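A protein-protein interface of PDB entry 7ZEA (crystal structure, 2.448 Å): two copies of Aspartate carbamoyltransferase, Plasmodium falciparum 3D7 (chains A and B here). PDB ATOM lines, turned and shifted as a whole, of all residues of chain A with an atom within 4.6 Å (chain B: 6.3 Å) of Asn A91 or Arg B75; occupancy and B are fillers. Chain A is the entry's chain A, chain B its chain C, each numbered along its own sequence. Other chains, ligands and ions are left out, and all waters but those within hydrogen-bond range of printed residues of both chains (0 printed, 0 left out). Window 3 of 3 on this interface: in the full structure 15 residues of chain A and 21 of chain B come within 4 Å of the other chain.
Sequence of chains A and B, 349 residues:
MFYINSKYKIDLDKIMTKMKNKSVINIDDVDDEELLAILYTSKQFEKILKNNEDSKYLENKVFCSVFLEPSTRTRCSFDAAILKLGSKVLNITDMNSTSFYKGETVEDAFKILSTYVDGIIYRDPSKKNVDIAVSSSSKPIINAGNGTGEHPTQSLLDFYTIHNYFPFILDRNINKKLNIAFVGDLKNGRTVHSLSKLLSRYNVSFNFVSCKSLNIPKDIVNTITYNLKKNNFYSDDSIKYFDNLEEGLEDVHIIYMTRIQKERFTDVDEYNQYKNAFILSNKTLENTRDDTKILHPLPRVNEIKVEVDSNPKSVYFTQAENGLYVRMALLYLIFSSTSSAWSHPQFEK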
ATOM      1  N   SER A  65     -19.042  25.170 -22.707  1.00  0.00           N
ATOM      2  CA  SER A  65     -20.344  25.573 -22.169  1.00  0.00           C
ATOM      3  C   SER A  65     -20.205  27.018 -21.697  1.00  0.00           C
ATOM      4  O   SER A  65     -19.358  27.270 -20.835  1.00  0.00           O
ATOM      5  CB  SER A  65     -20.770  24.614 -21.098  1.00  0.00           C
ATOM      6  OG  SER A  65     -21.763  25.189 -20.297  1.00  0.00           O
ATOM      7  N   ARG A  75     -27.271  24.167 -16.926  1.00  0.00           N
ATOM      8  CA  ARG A  75     -25.822  23.966 -17.177  1.00  0.00           C
ATOM      9  C   ARG A  75     -25.385  22.586 -16.644  1.00  0.00           C
ATOM     10  O   ARG A  75     -24.732  21.840 -17.393  1.00  0.00           O
ATOM     11  CB  ARG A  75     -25.010  25.162 -16.665  1.00  0.00           C
ATOM     12  CG  ARG A  75     -24.021  24.882 -15.569  1.00  0.00           C
ATOM     13  CD  ARG A  75     -22.657  25.307 -15.912  1.00  0.00           C
ATOM     14  NE  ARG A  75     -21.881  24.475 -15.031  1.00  0.00           N
ATOM     15  CZ  ARG A  75     -21.686  24.672 -13.729  1.00  0.00           C
ATOM     16  NH1 ARG A  75     -20.891  23.836 -13.101  1.00  0.00           N
ATOM     17  NH2 ARG A  75     -22.221  25.684 -13.059  1.00  0.00           N
ATOM     18  N   ASP A  79     -23.685  19.556 -18.680  1.00  0.00           N
ATOM     19  CA  ASP A  79     -22.359  19.045 -18.258  1.00  0.00           C
ATOM     20  C   ASP A  79     -22.475  17.535 -18.016  1.00  0.00           C
ATOM     21  O   ASP A  79     -21.627  16.751 -18.516  1.00  0.00           O
ATOM     22  CB  ASP A  79     -21.825  19.704 -16.975  1.00  0.00           C
ATOM     23  CG  ASP A  79     -21.197  21.089 -17.115  1.00  0.00           C
ATOM     24  OD1 ASP A  79     -20.981  21.571 -18.285  1.00  0.00           O
ATOM     25  OD2 ASP A  79     -20.964  21.708 -16.028  1.00  0.00           O
ATOM     26  N   VAL A  89     -15.644  18.852 -21.210  1.00  0.00           N
ATOM     27  CA  VAL A  89     -16.197  20.203 -21.315  1.00  0.00           C
ATOM     28  C   VAL A  89     -15.300  21.150 -20.494  1.00  0.00           C
ATOM     29  O   VAL A  89     -14.818  20.813 -19.378  1.00  0.00           O
ATOM     30  CB  VAL A  89     -17.671  20.222 -20.884  1.00  0.00           C
ATOM     31  CG1 VAL A  89     -17.876  19.691 -19.475  1.00  0.00           C
ATOM     32  CG2 VAL A  89     -18.257  21.616 -20.953  1.00  0.00           C
ATOM     33  N   LEU A  90     -15.233  22.341 -21.032  1.00  0.00           N
ATOM     34  CA  LEU A  90     -14.564  23.533 -20.525  1.00  0.00           C
ATOM     35  C   LEU A  90     -15.727  24.516 -20.318  1.00  0.00           C
ATOM     36  O   LEU A  90     -16.585  24.606 -21.214  1.00  0.00           O
ATOM     37  CB  LEU A  90     -13.573  23.655 -21.698  1.00  0.00           C
ATOM     38  CG  LEU A  90     -13.001  24.951 -22.171  1.00  0.00           C
ATOM     39  CD1 LEU A  90     -12.599  24.714 -23.603  1.00  0.00           C
ATOM     40  CD2 LEU A  90     -13.950  26.115 -22.055  1.00  0.00           C
ATOM     41  N   ASN A  91     -15.833  25.126 -19.147  1.00  0.00           N
ATOM     42  CA  ASN A  91     -17.009  25.893 -18.652  1.00  0.00           C
ATOM     43  C   ASN A  91     -16.666  27.379 -18.564  1.00  0.00           C
ATOM     44  O   ASN A  91     -15.605  27.693 -18.062  1.00  0.00           O
ATOM     45  CB  ASN A  91     -17.443  25.435 -17.260  1.00  0.00           C
ATOM     46  CG  ASN A  91     -18.129  24.092 -17.313  1.00  0.00           C
ATOM     47  OD1 ASN A  91     -19.336  23.963 -17.652  1.00  0.00           O
ATOM     48  ND2 ASN A  91     -17.338  23.074 -17.048  1.00  0.00           N
ATOM     49  N   ILE A  92     -17.548  28.260 -19.027  1.00  0.00           N
ATOM     50  CA  ILE A  92     -17.460  29.733 -18.792  1.00  0.00           C
ATOM     51  C   ILE A  92     -18.780  30.097 -18.133  1.00  0.00           C
ATOM     52  O   ILE A  92     -19.787  29.910 -18.842  1.00  0.00           O
ATOM     53  CB  ILE A  92     -17.247  30.482 -20.114  1.00  0.00           C
ATOM     54  CG1 ILE A  92     -16.004  30.031 -20.878  1.00  0.00           C
ATOM     55  CG2 ILE A  92     -17.241  31.960 -19.854  1.00  0.00           C
ATOM     56  CD1 ILE A  92     -15.863  30.649 -22.271  1.00  0.00           C
ATOM     57  N   THR A  93     -18.788  30.437 -16.835  1.00  0.00           N
ATOM     58  CA  THR A  93     -20.015  30.695 -16.030  1.00  0.00           C
ATOM     59  C   THR A  93     -19.832  31.983 -15.227  1.00  0.00           C
ATOM     60  O   THR A  93     -19.016  32.805 -15.613  1.00  0.00           O
ATOM     61  CB  THR A  93     -20.398  29.513 -15.115  1.00  0.00           C
ATOM     62  OG1 THR A  93     -19.531  29.515 -13.987  1.00  0.00           O
ATOM     63  CG2 THR A  93     -20.294  28.146 -15.755  1.00  0.00           C
ATOM     64  N   SER B  65      -5.280  24.576 -13.286  1.00  0.00           N
ATOM     65  CA  SER B  65      -5.208  25.863 -13.990  1.00  0.00           C
ATOM     66  C   SER B  65      -5.632  26.918 -12.983  1.00  0.00           C
ATOM     67  O   SER B  65      -6.742  26.803 -12.439  1.00  0.00           O
ATOM     68  CB  SER B  65      -6.043  25.819 -15.229  1.00  0.00           C
ATOM     69  OG  SER B  65      -6.397  27.128 -15.655  1.00  0.00           O
ATOM     70  N   PHE B  67      -5.999  30.900 -12.604  1.00  0.00           N
ATOM     71  CA  PHE B  67      -6.146  32.202 -13.289  1.00  0.00           C
ATOM     72  C   PHE B  67      -6.596  33.239 -12.247  1.00  0.00           C
ATOM     73  O   PHE B  67      -7.741  33.211 -11.862  1.00  0.00           O
ATOM     74  CB  PHE B  67      -7.079  32.007 -14.482  1.00  0.00           C
ATOM     75  CG  PHE B  67      -6.350  31.558 -15.722  1.00  0.00           C
ATOM     76  CD1 PHE B  67      -5.808  30.283 -15.766  1.00  0.00           C
ATOM     77  CD2 PHE B  67      -6.112  32.426 -16.792  1.00  0.00           C
ATOM     78  CE1 PHE B  67      -5.093  29.855 -16.866  1.00  0.00           C
ATOM     79  CE2 PHE B  67      -5.388  31.989 -17.891  1.00  0.00           C
ATOM     80  CZ  PHE B  67      -4.889  30.704 -17.929  1.00  0.00           C
ATOM     81  N   SER B  71      -8.768  36.074 -17.818  1.00  0.00           N
ATOM     82  CA  SER B  71      -8.166  36.033 -19.171  1.00  0.00           C
ATOM     83  C   SER B  71      -8.766  34.818 -19.860  1.00  0.00           C
ATOM     84  O   SER B  71      -8.051  33.810 -20.085  1.00  0.00           O
ATOM     85  CB  SER B  71      -6.638  36.031 -19.129  1.00  0.00           C
ATOM     86  OG  SER B  71      -6.053  36.100 -20.443  1.00  0.00           O
ATOM     87  N   THR B  72     -10.072  34.926 -20.097  1.00  0.00           N
ATOM     88  CA  THR B  72     -10.960  33.818 -20.522  1.00  0.00           C
ATOM     89  C   THR B  72     -10.428  33.189 -21.831  1.00  0.00           C
ATOM     90  O   THR B  72     -10.344  31.966 -21.920  1.00  0.00           O
ATOM     91  CB  THR B  72     -12.416  34.301 -20.511  1.00  0.00           C
ATOM     92  OG1 THR B  72     -12.751  34.736 -19.190  1.00  0.00           O
ATOM     93  CG2 THR B  72     -13.383  33.203 -20.876  1.00  0.00           C
ATOM     94  N   ARG B  73     -10.034  33.960 -22.816  1.00  0.00           N
ATOM     95  CA  ARG B  73      -9.520  33.373 -24.078  1.00  0.00           C
ATOM     96  C   ARG B  73      -8.334  32.454 -23.768  1.00  0.00           C
ATOM     97  O   ARG B  73      -8.280  31.368 -24.323  1.00  0.00           O
ATOM     98  CB  ARG B  73      -9.158  34.488 -25.070  1.00  0.00           C
ATOM     99  CG  ARG B  73      -8.707  34.011 -26.447  1.00  0.00           C
ATOM    100  CD  ARG B  73      -8.074  35.118 -27.355  1.00  0.00           C
ATOM    101  NE  ARG B  73      -8.998  36.241 -27.634  1.00  0.00           N
ATOM    102  CZ  ARG B  73      -9.230  37.291 -26.829  1.00  0.00           C
ATOM    103  NH1 ARG B  73     -10.175  38.159 -27.124  1.00  0.00           N
ATOM    104  NH2 ARG B  73      -8.567  37.453 -25.699  1.00  0.00           N
ATOM    105  N   THR B  74      -7.370  32.890 -22.954  1.00  0.00           N
ATOM    106  CA  THR B  74      -6.099  32.152 -22.713  1.00  0.00           C
ATOM    107  C   THR B  74      -6.431  30.930 -21.851  1.00  0.00           C
ATOM    108  O   THR B  74      -5.970  29.802 -22.156  1.00  0.00           O
ATOM    109  CB  THR B  74      -5.026  33.032 -22.055  1.00  0.00           C
ATOM    110  OG1 THR B  74      -4.917  34.216 -22.856  1.00  0.00           O
ATOM    111  CG2 THR B  74      -3.681  32.323 -21.917  1.00  0.00           C
ATOM    112  N   ARG B  75      -7.249  31.120 -20.836  1.00  0.00           N
ATOM    113  CA  ARG B  75      -7.648  29.988 -19.975  1.00  0.00           C
ATOM    114  C   ARG B  75      -8.344  28.895 -20.798  1.00  0.00           C
ATOM    115  O   ARG B  75      -7.928  27.704 -20.681  1.00  0.00           O
ATOM    116  CB  ARG B  75      -8.461  30.521 -18.811  1.00  0.00           C
ATOM    117  CG  ARG B  75      -9.051  29.404 -17.976  1.00  0.00           C
ATOM    118  CD  ARG B  75     -10.373  29.896 -17.435  1.00  0.00           C
ATOM    119  NE  ARG B  75     -11.325  28.942 -17.928  1.00  0.00           N
ATOM    120  CZ  ARG B  75     -12.627  29.087 -17.964  1.00  0.00           C
ATOM    121  NH1 ARG B  75     -13.308  28.065 -18.429  1.00  0.00           N
ATOM    122  NH2 ARG B  75     -13.249  30.202 -17.596  1.00  0.00           N
ATOM    123  N   CYS B  76      -9.288  29.262 -21.665  1.00  0.00           N
ATOM    124  CA  CYS B  76     -10.087  28.299 -22.462  1.00  0.00           C
ATOM    125  C   CYS B  76      -9.149  27.579 -23.431  1.00  0.00           C
ATOM    126  O   CYS B  76      -9.304  26.358 -23.679  1.00  0.00           O
ATOM    127  CB  CYS B  76     -11.235  29.013 -23.139  1.00  0.00           C
ATOM    128  SG  CYS B  76     -12.506  29.510 -21.949  1.00  0.00           S
ATOM    129  N   SER B  77      -8.152  28.267 -23.908  1.00  0.00           N
ATOM    130  CA  SER B  77      -7.200  27.705 -24.883  1.00  0.00           C
ATOM    131  C   SER B  77      -6.430  26.586 -24.190  1.00  0.00           C
ATOM    132  O   SER B  77      -6.206  25.487 -24.762  1.00  0.00           O
ATOM    133  CB  SER B  77      -6.290  28.828 -25.364  1.00  0.00           C
ATOM    134  OG  SER B  77      -5.381  28.331 -26.320  1.00  0.00           O
ATOM    135  N   PHE B  78      -5.967  26.863 -22.983  1.00  0.00           N
ATOM    136  CA  PHE B  78      -5.169  25.877 -22.217  1.00  0.00           C
ATOM    137  C   PHE B  78      -6.078  24.714 -21.826  1.00  0.00           C
ATOM    138  O   PHE B  78      -5.639  23.562 -21.968  1.00  0.00           O
ATOM    139  CB  PHE B  78      -4.522  26.559 -21.009  1.00  0.00           C
ATOM    140  CG  PHE B  78      -3.136  27.091 -21.242  1.00  0.00           C
ATOM    141  CD1 PHE B  78      -2.077  26.226 -21.401  1.00  0.00           C
ATOM    142  CD2 PHE B  78      -2.898  28.452 -21.220  1.00  0.00           C
ATOM    143  CE1 PHE B  78      -0.793  26.732 -21.543  1.00  0.00           C
ATOM    144  CE2 PHE B  78      -1.612  28.967 -21.342  1.00  0.00           C
ATOM    145  CZ  PHE B  78      -0.559  28.100 -21.514  1.00  0.00           C
ATOM    146  N   ASP B  79      -7.290  24.989 -21.343  1.00  0.00           N
ATOM    147  CA  ASP B  79      -8.241  23.912 -20.977  1.00  0.00           C
ATOM    148  C   ASP B  79      -8.425  22.997 -22.210  1.00  0.00           C
ATOM    149  O   ASP B  79      -8.351  21.760 -22.098  1.00  0.00           O
ATOM    150  CB  ASP B  79      -9.585  24.468 -20.505  1.00  0.00           C
ATOM    151  CG  ASP B  79      -9.654  24.975 -19.054  1.00  0.00           C
ATOM    152  OD1 ASP B  79      -8.660  24.789 -18.244  1.00  0.00           O
ATOM    153  OD2 ASP B  79     -10.734  25.583 -18.716  1.00  0.00           O
ATOM    154  N   ALA B  80      -8.652  23.602 -23.371  1.00  0.00           N
ATOM    155  CA  ALA B  80      -8.995  22.874 -24.596  1.00  0.00           C
ATOM    156  C   ALA B  80      -7.817  21.988 -24.959  1.00  0.00           C
ATOM    157  O   ALA B  80      -8.005  20.822 -25.341  1.00  0.00           O
ATOM    158  CB  ALA B  80      -9.337  23.849 -25.670  1.00  0.00           C
ATOM    159  N   ASN B  91      -9.840  23.658 -12.151  1.00  0.00           N
ATOM    160  CA  ASN B  91      -9.800  25.093 -12.457  1.00  0.00           C
ATOM    161  C   ASN B  91      -9.936  25.903 -11.174  1.00  0.00           C
ATOM    162  O   ASN B  91     -10.794  25.610 -10.355  1.00  0.00           O
ATOM    163  CB  ASN B  91     -10.936  25.455 -13.415  1.00  0.00           C
ATOM    164  CG  ASN B  91     -10.637  25.000 -14.837  1.00  0.00           C
ATOM    165  OD1 ASN B  91      -9.859  25.601 -15.617  1.00  0.00           O
ATOM    166  ND2 ASN B  91     -11.236  23.871 -15.148  1.00  0.00           N
ATOM    167  N   ILE B  92      -9.113  26.929 -11.029  1.00  0.00           N
ATOM    168  CA  ILE B  92      -9.310  28.028 -10.042  1.00  0.00           C
ATOM    169  C   ILE B  92      -9.357  29.289 -10.893  1.00  0.00           C
ATOM    170  O   ILE B  92      -8.346  29.555 -11.514  1.00  0.00           O
ATOM    171  CB  ILE B  92      -8.155  28.032  -9.029  1.00  0.00           C
ATOM    172  CG1 ILE B  92      -8.117  26.738  -8.227  1.00  0.00           C
ATOM    173  CG2 ILE B  92      -8.224  29.246  -8.131  1.00  0.00           C
ATOM    174  CD1 ILE B  92      -6.831  26.494  -7.528  1.00  0.00           C
ATOM    175  N   THR B  93     -10.515  29.933 -11.013  1.00  0.00           N
ATOM    176  CA  THR B  93     -10.758  31.156 -11.830  1.00  0.00           C
ATOM    177  C   THR B  93     -11.416  32.183 -10.915  1.00  0.00           C
ATOM    178  O   THR B  93     -11.028  32.161  -9.756  1.00  0.00           O
ATOM    179  CB  THR B  93     -11.596  30.857 -13.074  1.00  0.00           C
ATOM    180  OG1 THR B  93     -12.923  30.535 -12.669  1.00  0.00           O
ATOM    181  CG2 THR B  93     -11.051  29.717 -13.904  1.00  0.00           C
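The backbone carbonyl oxygen of Asn A91 sits close to the guanidinium group of Arg B75, 3.5 Å away.
N of Ser A65 is in hydrogen-bond range of O of Leu A90 (2.9 Å). O of Ser A65 is in hydrogen-bond range of N of Ile A92, 2.7 Å away. OD1 of Asn A91 sits close to OD1 of Asp A79 (3.0 Å). The backbone carbonyl oxygen of Thr B72 is in hydrogen-bond range of the side-chain sulfur of Cys B76. NE of Arg B75 is in salt-bridge range of OD2 of Asp B79. The side-chain amide oxygen (OD1) of Asn B91 lies close to the side-chain carboxylate (OD1) of Asp B79, 3.0 Å away.
Cys B76 touches Leu A90 (O to CD1, 3.7 Å). Asp B79 touches Leu A90. Leu A90 touches Ala B80. CD1 of Ile A92 touches CG2 of Thr B72, 3.8 Å away. Ile A92 touches Cys B76.
Of the printed residues of chain B, Leu A90 touches Cys B76 (3.7 Å), Asp B79 (3.8 Å) and Ala B80 (3.96 Å). Printed residues of chain B within 4 Å of Ile A92: Thr B72 and Cys B76. Of the printed residues of chain A, Thr B72 touches Ile A92. Thr B74 touches none of the printed residues of chain A. Printed residues of chain A within 4 Å of Arg B75: Asn A91 (2.4 Å). Of the printed residues of chain A, Cys B76 touches Leu A90 (3.7 Å) and Ile A92 (3.6 Å). The nearest printed residue of chain A that does not touch Ala B80 is Val A89 (7.6 Å).
Of the 15 printed residues of chain B, 5 touch a printed residue of chain A. Hydrophobic or aromatic side chains of chain B that line the printed part of chain A: Ala B80. Of the 8 printed residues of chain A, 3 touch a printed residue of chain B. Hydrophobic or aromatic side chains of chain A that line the printed part of chain B: Leu A90 and Ile A92. Among the printed residues, 6 pairs touch across the chains.
Asn A91 touches Arg B75, but with the chains exchanged Arg A75 does not touch Asn B91 (9.9 Å). 6 positions are printed for both chains.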
